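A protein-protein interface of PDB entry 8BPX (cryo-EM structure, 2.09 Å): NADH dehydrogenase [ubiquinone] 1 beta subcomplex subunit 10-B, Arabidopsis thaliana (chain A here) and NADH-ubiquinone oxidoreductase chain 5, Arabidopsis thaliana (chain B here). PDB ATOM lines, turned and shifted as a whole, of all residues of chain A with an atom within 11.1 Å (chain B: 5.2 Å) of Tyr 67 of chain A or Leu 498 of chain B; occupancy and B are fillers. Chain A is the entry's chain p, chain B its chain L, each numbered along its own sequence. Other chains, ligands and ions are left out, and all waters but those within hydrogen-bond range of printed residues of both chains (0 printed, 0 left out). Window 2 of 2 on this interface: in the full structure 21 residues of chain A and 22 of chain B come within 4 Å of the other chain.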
ATOM      1  N   VAL A  55      20.528 -11.880   6.587  1.00  0.00           N
ATOM      2  CA  VAL A  55      19.783 -12.834   5.744  1.00  0.00           C
ATOM      3  C   VAL A  55      19.301 -13.971   6.607  1.00  0.00           C
ATOM      4  O   VAL A  55      18.119 -14.216   6.516  1.00  0.00           O
ATOM      5  CB  VAL A  55      20.589 -13.276   4.498  1.00  0.00           C
ATOM      6  CG1 VAL A  55      19.927 -14.376   3.708  1.00  0.00           C
ATOM      7  CG2 VAL A  55      20.949 -12.096   3.614  1.00  0.00           C
ATOM      8  N   LYS A  56      20.196 -14.573   7.405  1.00  0.00           N
ATOM      9  CA  LYS A  56      19.869 -15.709   8.253  1.00  0.00           C
ATOM     10  C   LYS A  56      18.579 -15.351   9.032  1.00  0.00           C
ATOM     11  O   LYS A  56      17.610 -16.057   8.874  1.00  0.00           O
ATOM     12  CB  LYS A  56      21.046 -16.083   9.178  1.00  0.00           C
ATOM     13  CG  LYS A  56      20.896 -17.311  10.053  1.00  0.00           C
ATOM     14  CD  LYS A  56      22.076 -17.554  10.974  1.00  0.00           C
ATOM     15  CE  LYS A  56      23.342 -18.011  10.279  1.00  0.00           C
ATOM     16  NZ  LYS A  56      24.272 -16.911   9.931  1.00  0.00           N
ATOM     17  N   TRP A  57      18.622 -14.248   9.736  1.00  0.00           N
ATOM     18  CA  TRP A  57      17.511 -13.811  10.617  1.00  0.00           C
ATOM     19  C   TRP A  57      16.261 -13.368   9.863  1.00  0.00           C
ATOM     20  O   TRP A  57      15.245 -13.737  10.337  1.00  0.00           O
ATOM     21  CB  TRP A  57      18.027 -12.823  11.650  1.00  0.00           C
ATOM     22  CG  TRP A  57      18.812 -13.600  12.660  1.00  0.00           C
ATOM     23  CD1 TRP A  57      20.163 -13.575  12.851  1.00  0.00           C
ATOM     24  CD2 TRP A  57      18.306 -14.624  13.534  1.00  0.00           C
ATOM     25  NE1 TRP A  57      20.518 -14.472  13.814  1.00  0.00           N
ATOM     26  CE2 TRP A  57      19.406 -15.127  14.261  1.00  0.00           C
ATOM     27  CE3 TRP A  57      17.034 -15.146  13.795  1.00  0.00           C
ATOM     28  CZ2 TRP A  57      19.275 -16.128  15.220  1.00  0.00           C
ATOM     29  CZ3 TRP A  57      16.905 -16.132  14.743  1.00  0.00           C
ATOM     30  CH2 TRP A  57      18.009 -16.609  15.457  1.00  0.00           C
ATOM     31  N   CYS A  58      16.387 -12.719   8.707  1.00  0.00           N
ATOM     32  CA  CYS A  58      15.210 -12.324   7.890  1.00  0.00           C
ATOM     33  C   CYS A  58      14.493 -13.594   7.405  1.00  0.00           C
ATOM     34  O   CYS A  58      13.335 -13.687   7.709  1.00  0.00           O
ATOM     35  CB  CYS A  58      15.610 -11.294   6.840  1.00  0.00           C
ATOM     36  SG  CYS A  58      14.282 -10.687   5.776  1.00  0.00           S
ATOM     37  N   TYR A  59      15.193 -14.571   6.817  1.00  0.00           N
ATOM     38  CA  TYR A  59      14.637 -15.887   6.473  1.00  0.00           C
ATOM     39  C   TYR A  59      13.863 -16.426   7.668  1.00  0.00           C
ATOM     40  O   TYR A  59      12.728 -16.752   7.442  1.00  0.00           O
ATOM     41  CB  TYR A  59      15.678 -16.889   5.930  1.00  0.00           C
ATOM     42  CG  TYR A  59      15.158 -18.174   5.373  1.00  0.00           C
ATOM     43  CD1 TYR A  59      14.799 -18.256   4.041  1.00  0.00           C
ATOM     44  CD2 TYR A  59      15.055 -19.300   6.168  1.00  0.00           C
ATOM     45  CE1 TYR A  59      14.341 -19.435   3.506  1.00  0.00           C
ATOM     46  CE2 TYR A  59      14.599 -20.493   5.644  1.00  0.00           C
ATOM     47  CZ  TYR A  59      14.239 -20.551   4.312  1.00  0.00           C
ATOM     48  OH  TYR A  59      13.782 -21.694   3.754  1.00  0.00           O
ATOM     49  N   ARG A  60      14.494 -16.519   8.826  1.00  0.00           N
ATOM     50  CA  ARG A  60      13.920 -17.074  10.051  1.00  0.00           C
ATOM     51  C   ARG A  60      12.735 -16.240  10.545  1.00  0.00           C
ATOM     52  O   ARG A  60      11.831 -16.796  11.063  1.00  0.00           O
ATOM     53  CB  ARG A  60      15.005 -17.167  11.132  1.00  0.00           C
ATOM     54  CG  ARG A  60      16.028 -18.266  10.884  1.00  0.00           C
ATOM     55  CD  ARG A  60      17.268 -18.217  11.738  1.00  0.00           C
ATOM     56  NE  ARG A  60      18.160 -19.307  11.380  1.00  0.00           N
ATOM     57  CZ  ARG A  60      19.200 -19.707  12.096  1.00  0.00           C
ATOM     58  NH1 ARG A  60      19.515 -19.104  13.224  1.00  0.00           N
ATOM     59  NH2 ARG A  60      19.925 -20.715  11.670  1.00  0.00           N
ATOM     60  N   VAL A  61      12.868 -14.932  10.468  1.00  0.00           N
ATOM     61  CA  VAL A  61      11.770 -14.162  11.037  1.00  0.00           C
ATOM     62  C   VAL A  61      10.595 -14.080  10.066  1.00  0.00           C
ATOM     63  O   VAL A  61       9.436 -14.187  10.471  1.00  0.00           O
ATOM     64  CB  VAL A  61      12.269 -12.767  11.465  1.00  0.00           C
ATOM     65  CG1 VAL A  61      11.116 -11.782  11.589  1.00  0.00           C
ATOM     66  CG2 VAL A  61      13.031 -12.858  12.779  1.00  0.00           C
ATOM     67  N   GLU A  62      10.864 -13.915   8.774  1.00  0.00           N
ATOM     68  CA  GLU A  62       9.801 -13.643   7.815  1.00  0.00           C
ATOM     69  C   GLU A  62       9.152 -14.889   7.226  1.00  0.00           C
ATOM     70  O   GLU A  62       8.096 -14.768   6.599  1.00  0.00           O
ATOM     71  CB  GLU A  62      10.332 -12.760   6.685  1.00  0.00           C
ATOM     72  CG  GLU A  62      10.978 -11.483   7.171  1.00  0.00           C
ATOM     73  CD  GLU A  62       9.976 -10.448   7.659  1.00  0.00           C
ATOM     74  OE1 GLU A  62       8.788 -10.776   7.823  1.00  0.00           O
ATOM     75  OE2 GLU A  62      10.386  -9.295   7.884  1.00  0.00           O
ATOM     76  N   GLY A  63       9.746 -16.065   7.408  1.00  0.00           N
ATOM     77  CA  GLY A  63       9.119 -17.293   6.942  1.00  0.00           C
ATOM     78  C   GLY A  63       8.866 -17.285   5.446  1.00  0.00           C
ATOM     79  O   GLY A  63       9.753 -16.993   4.642  1.00  0.00           O
ATOM     80  N   VAL A  64       7.702 -17.735   5.010  1.00  0.00           N
ATOM     81  CA  VAL A  64       7.246 -17.698   3.581  1.00  0.00           C
ATOM     82  C   VAL A  64       7.251 -16.297   2.952  1.00  0.00           C
ATOM     83  O   VAL A  64       7.253 -16.262   1.753  1.00  0.00           O
ATOM     84  CB  VAL A  64       5.857 -18.382   3.438  1.00  0.00           C
ATOM     85  CG1 VAL A  64       5.911 -19.854   3.835  1.00  0.00           C
ATOM     86  CG2 VAL A  64       4.778 -17.643   4.221  1.00  0.00           C
ATOM     87  N   ASN A  65       7.340 -15.222   3.706  1.00  0.00           N
ATOM     88  CA  ASN A  65       7.467 -13.894   3.120  1.00  0.00           C
ATOM     89  C   ASN A  65       8.922 -13.484   2.896  1.00  0.00           C
ATOM     90  O   ASN A  65       9.182 -12.327   2.546  1.00  0.00           O
ATOM     91  CB  ASN A  65       6.761 -12.852   3.995  1.00  0.00           C
ATOM     92  CG  ASN A  65       5.306 -13.197   4.261  1.00  0.00           C
ATOM     93  OD1 ASN A  65       4.580 -13.611   3.363  1.00  0.00           O
ATOM     94  ND2 ASN A  65       4.877 -13.025   5.500  1.00  0.00           N
ATOM     95  N   HIS A  66       9.869 -14.409   3.079  1.00  0.00           N
ATOM     96  CA  HIS A  66      11.283 -14.062   2.988  1.00  0.00           C
ATOM     97  C   HIS A  66      11.676 -13.597   1.589  1.00  0.00           C
ATOM     98  O   HIS A  66      12.547 -12.737   1.454  1.00  0.00           O
ATOM     99  CB  HIS A  66      12.142 -15.252   3.422  1.00  0.00           C
ATOM    100  CG  HIS A  66      12.270 -16.318   2.382  1.00  0.00           C
ATOM    101  ND1 HIS A  66      13.182 -16.251   1.354  1.00  0.00           N
ATOM    102  CD2 HIS A  66      11.607 -17.486   2.220  1.00  0.00           C
ATOM    103  CE1 HIS A  66      13.070 -17.326   0.598  1.00  0.00           C
ATOM    104  NE2 HIS A  66      12.123 -18.092   1.102  1.00  0.00           N
ATOM    105  N   TYR A  67      11.042 -14.141   0.546  1.00  0.00           N
ATOM    106  CA  TYR A  67      11.399 -13.756  -0.817  1.00  0.00           C
ATOM    107  C   TYR A  67      11.219 -12.261  -1.037  1.00  0.00           C
ATOM    108  O   TYR A  67      12.068 -11.607  -1.653  1.00  0.00           O
ATOM    109  CB  TYR A  67      10.551 -14.525  -1.827  1.00  0.00           C
ATOM    110  CG  TYR A  67      11.000 -15.937  -2.117  1.00  0.00           C
ATOM    111  CD1 TYR A  67      12.285 -16.206  -2.573  1.00  0.00           C
ATOM    112  CD2 TYR A  67      10.127 -16.999  -1.954  1.00  0.00           C
ATOM    113  CE1 TYR A  67      12.685 -17.503  -2.847  1.00  0.00           C
ATOM    114  CE2 TYR A  67      10.510 -18.288  -2.225  1.00  0.00           C
ATOM    115  CZ  TYR A  67      11.788 -18.538  -2.669  1.00  0.00           C
ATOM    116  OH  TYR A  67      12.161 -19.831  -2.935  1.00  0.00           O
ATOM    117  N   GLN A  68      10.118 -11.702  -0.545  1.00  0.00           N
ATOM    118  CA  GLN A  68       9.854 -10.283  -0.714  1.00  0.00           C
ATOM    119  C   GLN A  68      10.495  -9.441   0.378  1.00  0.00           C
ATOM    120  O   GLN A  68      10.864  -8.292   0.124  1.00  0.00           O
ATOM    121  CB  GLN A  68       8.337 -10.046  -0.781  1.00  0.00           C
ATOM    122  CG  GLN A  68       7.828  -8.742  -0.199  1.00  0.00           C
ATOM    123  CD  GLN A  68       6.344  -8.535  -0.466  1.00  0.00           C
ATOM    124  OE1 GLN A  68       5.524  -9.415  -0.204  1.00  0.00           O
ATOM    125  NE2 GLN A  68       5.996  -7.372  -1.001  1.00  0.00           N
ATOM    126  N   LYS A  69      10.688  -9.996   1.576  1.00  0.00           N
ATOM    127  CA  LYS A  69      11.275  -9.219   2.661  1.00  0.00           C
ATOM    128  C   LYS A  69      12.803  -9.232   2.672  1.00  0.00           C
ATOM    129  O   LYS A  69      13.408  -8.224   3.044  1.00  0.00           O
ATOM    130  CB  LYS A  69      10.752  -9.712   4.012  1.00  0.00           C
ATOM    131  CG  LYS A  69       9.243  -9.582   4.174  1.00  0.00           C
ATOM    132  CD  LYS A  69       8.810  -8.129   4.147  1.00  0.00           C
ATOM    133  CE  LYS A  69       7.317  -7.967   4.379  1.00  0.00           C
ATOM    134  NZ  LYS A  69       6.879  -6.544   4.331  1.00  0.00           N
ATOM    135  N   CYS A  70      13.445 -10.335   2.283  1.00  0.00           N
ATOM    136  CA  CYS A  70      14.903 -10.438   2.319  1.00  0.00           C
ATOM    137  C   CYS A  70      15.578  -9.926   1.058  1.00  0.00           C
ATOM    138  O   CYS A  70      16.810  -9.954   0.987  1.00  0.00           O
ATOM    139  CB  CYS A  70      15.357 -11.892   2.530  1.00  0.00           C
ATOM    140  SG  CYS A  70      14.553 -12.834   3.822  1.00  0.00           S
ATOM    141  N   ARG A  71      14.808  -9.462   0.073  1.00  0.00           N
ATOM    142  CA  ARG A  71      15.340  -9.248  -1.271  1.00  0.00           C
ATOM    143  C   ARG A  71      16.543  -8.310  -1.263  1.00  0.00           C
ATOM    144  O   ARG A  71      17.586  -8.616  -1.854  1.00  0.00           O
ATOM    145  CB  ARG A  71      14.226  -8.710  -2.166  1.00  0.00           C
ATOM    146  CG  ARG A  71      14.660  -8.213  -3.506  1.00  0.00           C
ATOM    147  CD  ARG A  71      13.471  -8.150  -4.444  1.00  0.00           C
ATOM    148  NE  ARG A  71      13.846  -8.415  -5.825  1.00  0.00           N
ATOM    149  CZ  ARG A  71      14.223  -7.476  -6.682  1.00  0.00           C
ATOM    150  NH1 ARG A  71      14.303  -6.207  -6.322  1.00  0.00           N
ATOM    151  NH2 ARG A  71      14.521  -7.822  -7.929  1.00  0.00           N
ATOM    152  N   HIS A  72      16.422  -7.169  -0.582  1.00  0.00           N
ATOM    153  CA  HIS A  72      17.523  -6.213  -0.538  1.00  0.00           C
ATOM    154  C   HIS A  72      18.709  -6.763   0.253  1.00  0.00           C
ATOM    155  O   HIS A  72      19.866  -6.572  -0.142  1.00  0.00           O
ATOM    156  CB  HIS A  72      17.023  -4.871   0.016  1.00  0.00           C
ATOM    157  CG  HIS A  72      16.796  -4.847   1.499  1.00  0.00           C
ATOM    158  ND1 HIS A  72      15.559  -4.597   2.051  1.00  0.00           N
ATOM    159  CD2 HIS A  72      17.653  -4.957   2.543  1.00  0.00           C
ATOM    160  CE1 HIS A  72      15.655  -4.607   3.368  1.00  0.00           C
ATOM    161  NE2 HIS A  72      16.914  -4.826   3.692  1.00  0.00           N
ATOM    162  N   LEU A  73      18.445  -7.464   1.357  1.00  0.00           N
ATOM    163  CA  LEU A  73      19.530  -8.065   2.128  1.00  0.00           C
ATOM    164  C   LEU A  73      20.231  -9.155   1.330  1.00  0.00           C
ATOM    165  O   LEU A  73      21.461  -9.267   1.372  1.00  0.00           O
ATOM    166  CB  LEU A  73      18.997  -8.622   3.445  1.00  0.00           C
ATOM    167  CG  LEU A  73      18.652  -7.596   4.524  1.00  0.00           C
ATOM    168  CD1 LEU A  73      18.196  -8.285   5.797  1.00  0.00           C
ATOM    169  CD2 LEU A  73      19.832  -6.673   4.794  1.00  0.00           C
ATOM    170  N   VAL A  74      19.463  -9.964   0.594  1.00  0.00           N
ATOM    171  CA  VAL A  74      20.060 -11.003  -0.235  1.00  0.00           C
ATOM    172  C   VAL A  74      20.941 -10.378  -1.307  1.00  0.00           C
ATOM    173  O   VAL A  74      22.056 -10.848  -1.566  1.00  0.00           O
ATOM    174  CB  VAL A  74      18.969 -11.899  -0.850  1.00  0.00           C
ATOM    175  CG1 VAL A  74      19.552 -12.775  -1.950  1.00  0.00           C
ATOM    176  CG2 VAL A  74      18.313 -12.748   0.218  1.00  0.00           C
ATOM    177  N   GLN A  75      20.454  -9.310  -1.943  1.00  0.00           N
ATOM    178  CA  GLN A  75      21.253  -8.635  -2.959  1.00  0.00           C
ATOM    179  C   GLN A  75      22.546  -8.088  -2.363  1.00  0.00           C
ATOM    180  O   GLN A  75      23.622  -8.241  -2.953  1.00  0.00           O
ATOM    181  CB  GLN A  75      20.411  -7.539  -3.627  1.00  0.00           C
ATOM    182  CG  GLN A  75      21.142  -6.407  -4.344  1.00  0.00           C
ATOM    183  CD  GLN A  75      21.824  -5.415  -3.413  1.00  0.00           C
ATOM    184  OE1 GLN A  75      21.244  -4.975  -2.421  1.00  0.00           O
ATOM    185  NE2 GLN A  75      23.067  -5.069  -3.726  1.00  0.00           N
ATOM    186  N   LEU A  78      24.964 -11.070  -1.558  1.00  0.00           N
ATOM    187  CA  LEU A  78      25.535 -11.692  -2.746  1.00  0.00           C
ATOM    188  C   LEU A  78      26.507 -10.757  -3.452  1.00  0.00           C
ATOM    189  O   LEU A  78      27.501 -11.221  -4.023  1.00  0.00           O
ATOM    190  CB  LEU A  78      24.422 -12.144  -3.687  1.00  0.00           C
ATOM    191  CG  LEU A  78      23.688 -13.421  -3.270  1.00  0.00           C
ATOM    192  CD1 LEU A  78      22.753 -13.883  -4.364  1.00  0.00           C
ATOM    193  CD2 LEU A  78      24.668 -14.531  -2.897  1.00  0.00           C
ATOM    194  N   PHE B 198      18.981 -21.084   1.556  1.00  0.00           N
ATOM    195  CA  PHE B 198      17.598 -21.095   1.094  1.00  0.00           C
ATOM    196  C   PHE B 198      17.093 -19.690   0.797  1.00  0.00           C
ATOM    197  O   PHE B 198      16.266 -19.511  -0.103  1.00  0.00           O
ATOM    198  CB  PHE B 198      16.693 -21.789   2.114  1.00  0.00           C
ATOM    199  CG  PHE B 198      17.086 -23.208   2.405  1.00  0.00           C
ATOM    200  CD1 PHE B 198      17.761 -23.963   1.454  1.00  0.00           C
ATOM    201  CD2 PHE B 198      16.770 -23.795   3.615  1.00  0.00           C
ATOM    202  CE1 PHE B 198      18.130 -25.263   1.719  1.00  0.00           C
ATOM    203  CE2 PHE B 198      17.131 -25.093   3.883  1.00  0.00           C
ATOM    204  CZ  PHE B 198      17.811 -25.832   2.932  1.00  0.00           C
ATOM    205  N   SER B 202      17.225 -18.620  -5.152  1.00  0.00           N
ATOM    206  CA  SER B 202      16.505 -18.262  -6.365  1.00  0.00           C
ATOM    207  C   SER B 202      17.303 -17.351  -7.288  1.00  0.00           C
ATOM    208  O   SER B 202      16.939 -17.212  -8.459  1.00  0.00           O
ATOM    209  CB  SER B 202      15.172 -17.602  -6.005  1.00  0.00           C
ATOM    210  OG  SER B 202      15.329 -16.224  -5.737  1.00  0.00           O
ATOM    211  N   SER B 273      14.510 -28.795  -0.272  1.00  0.00           N
ATOM    212  CA  SER B 273      13.548 -28.349  -1.282  1.00  0.00           C
ATOM    213  C   SER B 273      13.660 -26.876  -1.680  1.00  0.00           C
ATOM    214  O   SER B 273      13.456 -26.583  -2.869  1.00  0.00           O
ATOM    215  CB  SER B 273      12.111 -28.665  -0.833  1.00  0.00           C
ATOM    216  OG  SER B 273      11.741 -27.990   0.353  1.00  0.00           O
ATOM    217  N   PRO B 274      13.969 -25.917  -0.794  1.00  0.00           N
ATOM    218  CA  PRO B 274      14.169 -24.539  -1.278  1.00  0.00           C
ATOM    219  C   PRO B 274      15.319 -24.405  -2.259  1.00  0.00           C
ATOM    220  O   PRO B 274      15.373 -23.416  -2.998  1.00  0.00           O
ATOM    221  CB  PRO B 274      14.430 -23.744   0.008  1.00  0.00           C
ATOM    222  CG  PRO B 274      13.811 -24.545   1.074  1.00  0.00           C
ATOM    223  CD  PRO B 274      14.048 -25.965   0.676  1.00  0.00           C
ATOM    224  N   GLU B 277      14.059 -26.881  -5.696  1.00  0.00           N
ATOM    225  CA  GLU B 277      12.966 -26.348  -6.498  1.00  0.00           C
ATOM    226  C   GLU B 277      13.456 -25.537  -7.689  1.00  0.00           C
ATOM    227  O   GLU B 277      12.707 -25.369  -8.655  1.00  0.00           O
ATOM    228  CB  GLU B 277      12.044 -25.489  -5.631  1.00  0.00           C
ATOM    229  CG  GLU B 277      10.919 -26.266  -4.985  1.00  0.00           C
ATOM    230  CD  GLU B 277      10.007 -26.938  -5.988  1.00  0.00           C
ATOM    231  OE1 GLU B 277       9.259 -26.228  -6.691  1.00  0.00           O
ATOM    232  OE2 GLU B 277      10.035 -28.182  -6.074  1.00  0.00           O
ATOM    233  N   TYR B 278      14.690 -25.041  -7.657  1.00  0.00           N
ATOM    234  CA  TYR B 278      15.253 -24.299  -8.775  1.00  0.00           C
ATOM    235  C   TYR B 278      16.156 -25.156  -9.651  1.00  0.00           C
ATOM    236  O   TYR B 278      17.015 -24.621 -10.358  1.00  0.00           O
ATOM    237  CB  TYR B 278      15.981 -23.053  -8.271  1.00  0.00           C
ATOM    238  CG  TYR B 278      15.065 -22.124  -7.515  1.00  0.00           C
ATOM    239  CD1 TYR B 278      14.297 -21.178  -8.193  1.00  0.00           C
ATOM    240  CD2 TYR B 278      14.954 -22.189  -6.135  1.00  0.00           C
ATOM    241  CE1 TYR B 278      13.441 -20.335  -7.517  1.00  0.00           C
ATOM    242  CE2 TYR B 278      14.105 -21.347  -5.448  1.00  0.00           C
ATOM    243  CZ  TYR B 278      13.349 -20.423  -6.144  1.00  0.00           C
ATOM    244  OH  TYR B 278      12.507 -19.581  -5.467  1.00  0.00           O
ATOM    245  N   TYR B 331       6.804 -32.603  -1.505  1.00  0.00           N
ATOM    246  CA  TYR B 331       7.645 -33.027  -0.390  1.00  0.00           C
ATOM    247  C   TYR B 331       6.832 -33.321   0.859  1.00  0.00           C
ATOM    248  O   TYR B 331       7.181 -34.232   1.619  1.00  0.00           O
ATOM    249  CB  TYR B 331       8.693 -31.959  -0.080  1.00  0.00           C
ATOM    250  CG  TYR B 331       9.439 -31.458  -1.287  1.00  0.00           C
ATOM    251  CD1 TYR B 331      10.536 -32.151  -1.786  1.00  0.00           C
ATOM    252  CD2 TYR B 331       9.054 -30.288  -1.930  1.00  0.00           C
ATOM    253  CE1 TYR B 331      11.221 -31.697  -2.891  1.00  0.00           C
ATOM    254  CE2 TYR B 331       9.733 -29.827  -3.033  1.00  0.00           C
ATOM    255  CZ  TYR B 331      10.818 -30.532  -3.510  1.00  0.00           C
ATOM    256  OH  TYR B 331      11.499 -30.074  -4.608  1.00  0.00           O
ATOM    257  N   SER B 496       9.301 -24.642   6.279  1.00  0.00           N
ATOM    258  CA  SER B 496      10.220 -25.776   6.213  1.00  0.00           C
ATOM    259  C   SER B 496      10.296 -26.355   4.807  1.00  0.00           C
ATOM    260  O   SER B 496      11.373 -26.747   4.348  1.00  0.00           O
ATOM    261  CB  SER B 496       9.800 -26.853   7.211  1.00  0.00           C
ATOM    262  OG  SER B 496       9.619 -26.313   8.502  1.00  0.00           O
ATOM    263  N   LEU B 497       9.168 -26.421   4.109  1.00  0.00           N
ATOM    264  CA  LEU B 497       9.108 -26.954   2.759  1.00  0.00           C
ATOM    265  C   LEU B 497       8.711 -25.849   1.793  1.00  0.00           C
ATOM    266  O   LEU B 497       7.987 -24.918   2.152  1.00  0.00           O
ATOM    267  CB  LEU B 497       8.120 -28.122   2.664  1.00  0.00           C
ATOM    268  CG  LEU B 497       8.353 -29.248   3.674  1.00  0.00           C
ATOM    269  CD1 LEU B 497       7.180 -30.205   3.699  1.00  0.00           C
ATOM    270  CD2 LEU B 497       9.646 -29.981   3.356  1.00  0.00           C
ATOM    271  N   LEU B 498       9.216 -25.948   0.565  1.00  0.00           N
ATOM    272  CA  LEU B 498       8.933 -24.974  -0.479  1.00  0.00           C
ATOM    273  C   LEU B 498       8.429 -25.687  -1.722  1.00  0.00           C
ATOM    274  O   LEU B 498       9.105 -26.572  -2.253  1.00  0.00           O
ATOM    275  CB  LEU B 498      10.169 -24.139  -0.819  1.00  0.00           C
ATOM    276  CG  LEU B 498       9.938 -23.142  -1.960  1.00  0.00           C
ATOM    277  CD1 LEU B 498       9.377 -21.821  -1.437  1.00  0.00           C
ATOM    278  CD2 LEU B 498      11.209 -22.920  -2.758  1.00  0.00           C
ATOM    279  N   VAL B 499       7.245 -25.299  -2.182  1.00  0.00           N
ATOM    280  CA  VAL B 499       6.734 -25.663  -3.497  1.00  0.00           C
ATOM    281  C   VAL B 499       6.475 -24.367  -4.243  1.00  0.00           C
ATOM    282  O   VAL B 499       5.682 -23.534  -3.789  1.00  0.00           O
ATOM    283  CB  VAL B 499       5.454 -26.510  -3.413  1.00  0.00           C
ATOM    284  CG1 VAL B 499       5.079 -27.056  -4.787  1.00  0.00           C
ATOM    285  CG2 VAL B 499       5.628 -27.637  -2.424  1.00  0.00           C
ATOM    286  N   LEU B 500       7.160 -24.216  -5.358  1.00  0.00           N
ATOM    287  CA  LEU B 500       6.922 -23.048  -6.216  1.00  0.00           C
ATOM    288  C   LEU B 500       5.509 -23.141  -6.784  1.00  0.00           C
ATOM    289  O   LEU B 500       5.092 -24.260  -7.110  1.00  0.00           O
ATOM    290  CB  LEU B 500       7.965 -23.030  -7.328  1.00  0.00           C
ATOM    291  CG  LEU B 500       9.390 -22.676  -6.891  1.00  0.00           C
ATOM    292  CD1 LEU B 500      10.366 -22.788  -8.045  1.00  0.00           C
ATOM    293  CD2 LEU B 500       9.459 -21.293  -6.270  1.00  0.00           C
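The backbone NH (N) of Leu 498 of chain B lies within hydrogen-bond range of the side-chain hydroxyl (OG) of Ser 273 of chain B, at 3.3 Å.
SG of Cys 70 of chain A sits at hydrogen-bond distance from N of Tyr 59 of chain A, at 3.5 Å.
The side-chain sulfur of Cys 70 of chain A is in hydrogen-bond range of the backbone carbonyl oxygen of His 66 of chain A (3.1 Å).
Cys 58 of chain A touches none of the printed residues of chain B.
Of the printed residues of chain B, Tyr 59 of chain A touches Phe 198 (3.3 Å) and Pro 274 (3.9 Å).
Of the printed residues of chain B, His 66 of chain A touches Phe 198.
Of chain B, only Tyr 278 (2.6 Å) and Leu 498 (3.2 Å) come within 4 Å of Tyr 67 of chain A.
Printed residues of chain A within 4 Å of Phe 198 of chain B: Tyr 59 (3.3 Å) and His 66 (3.9 Å).
No residue of chain A comes within 4 Å of Ser 202 of chain B.
No residue of chain A comes within 4 Å of Ser 273 of chain B.
Of the printed residues of chain A, Pro 274 of chain B touches Tyr 59.
No residue of chain A comes within 4 Å of Glu 277 of chain B.
Printed residues of chain A within 4 Å of Tyr 278 of chain B: Tyr 67 (2.6 Å).
Tyr 331 of chain B touches none of the printed residues of chain A.
Leu 498 of chain B touches just one residue of chain A: Tyr 67 (3.2 Å).
The nearest residue of chain B that does not touch Tyr 67 of chain A is Ser 202 of chain B (4.02 Å).
The nearest printed residue of chain A that does not touch Phe 198 of chain B is Tyr 67 of chain A (4.9 Å).
OH of Tyr 59 of chain A touches CB of Phe 198 of chain B, at 3.3 Å.
CG of Pro 274 of chain B touches OH of Tyr 59 of chain A (3.9 Å).
His 66 of chain A touches Phe 198 of chain B (CE1 to O, 3.9 Å).
Leu 498 of chain B touches Tyr 67 of chain A.
Hydrophobic or aromatic side chains of chain B within 4 Å of the printed part of chain A: Phe 198, Pro 274, Tyr 278 and Leu 498.
Of the 22 printed residues of chain A, 3 touch a printed residue of chain B.
Hydrophobic or aromatic side chains of chain A within 4 Å of the printed part of chain B: Tyr 59, His 66 and Tyr 67.
Along chain A the printed residues that touch a printed residue of chain B span positions 59 to 67.
Among the printed residues, 5 pairs touch across the chains.
Among the printed residues, no Asp or Glu carboxylate lies within 4 Å of a Lys or Arg side-chain nitrogen of the other chain.
OH of Tyr 278 of chain B sits at hydrogen-bond distance from OH of Tyr 67 of chain A, at 2.6 Å.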
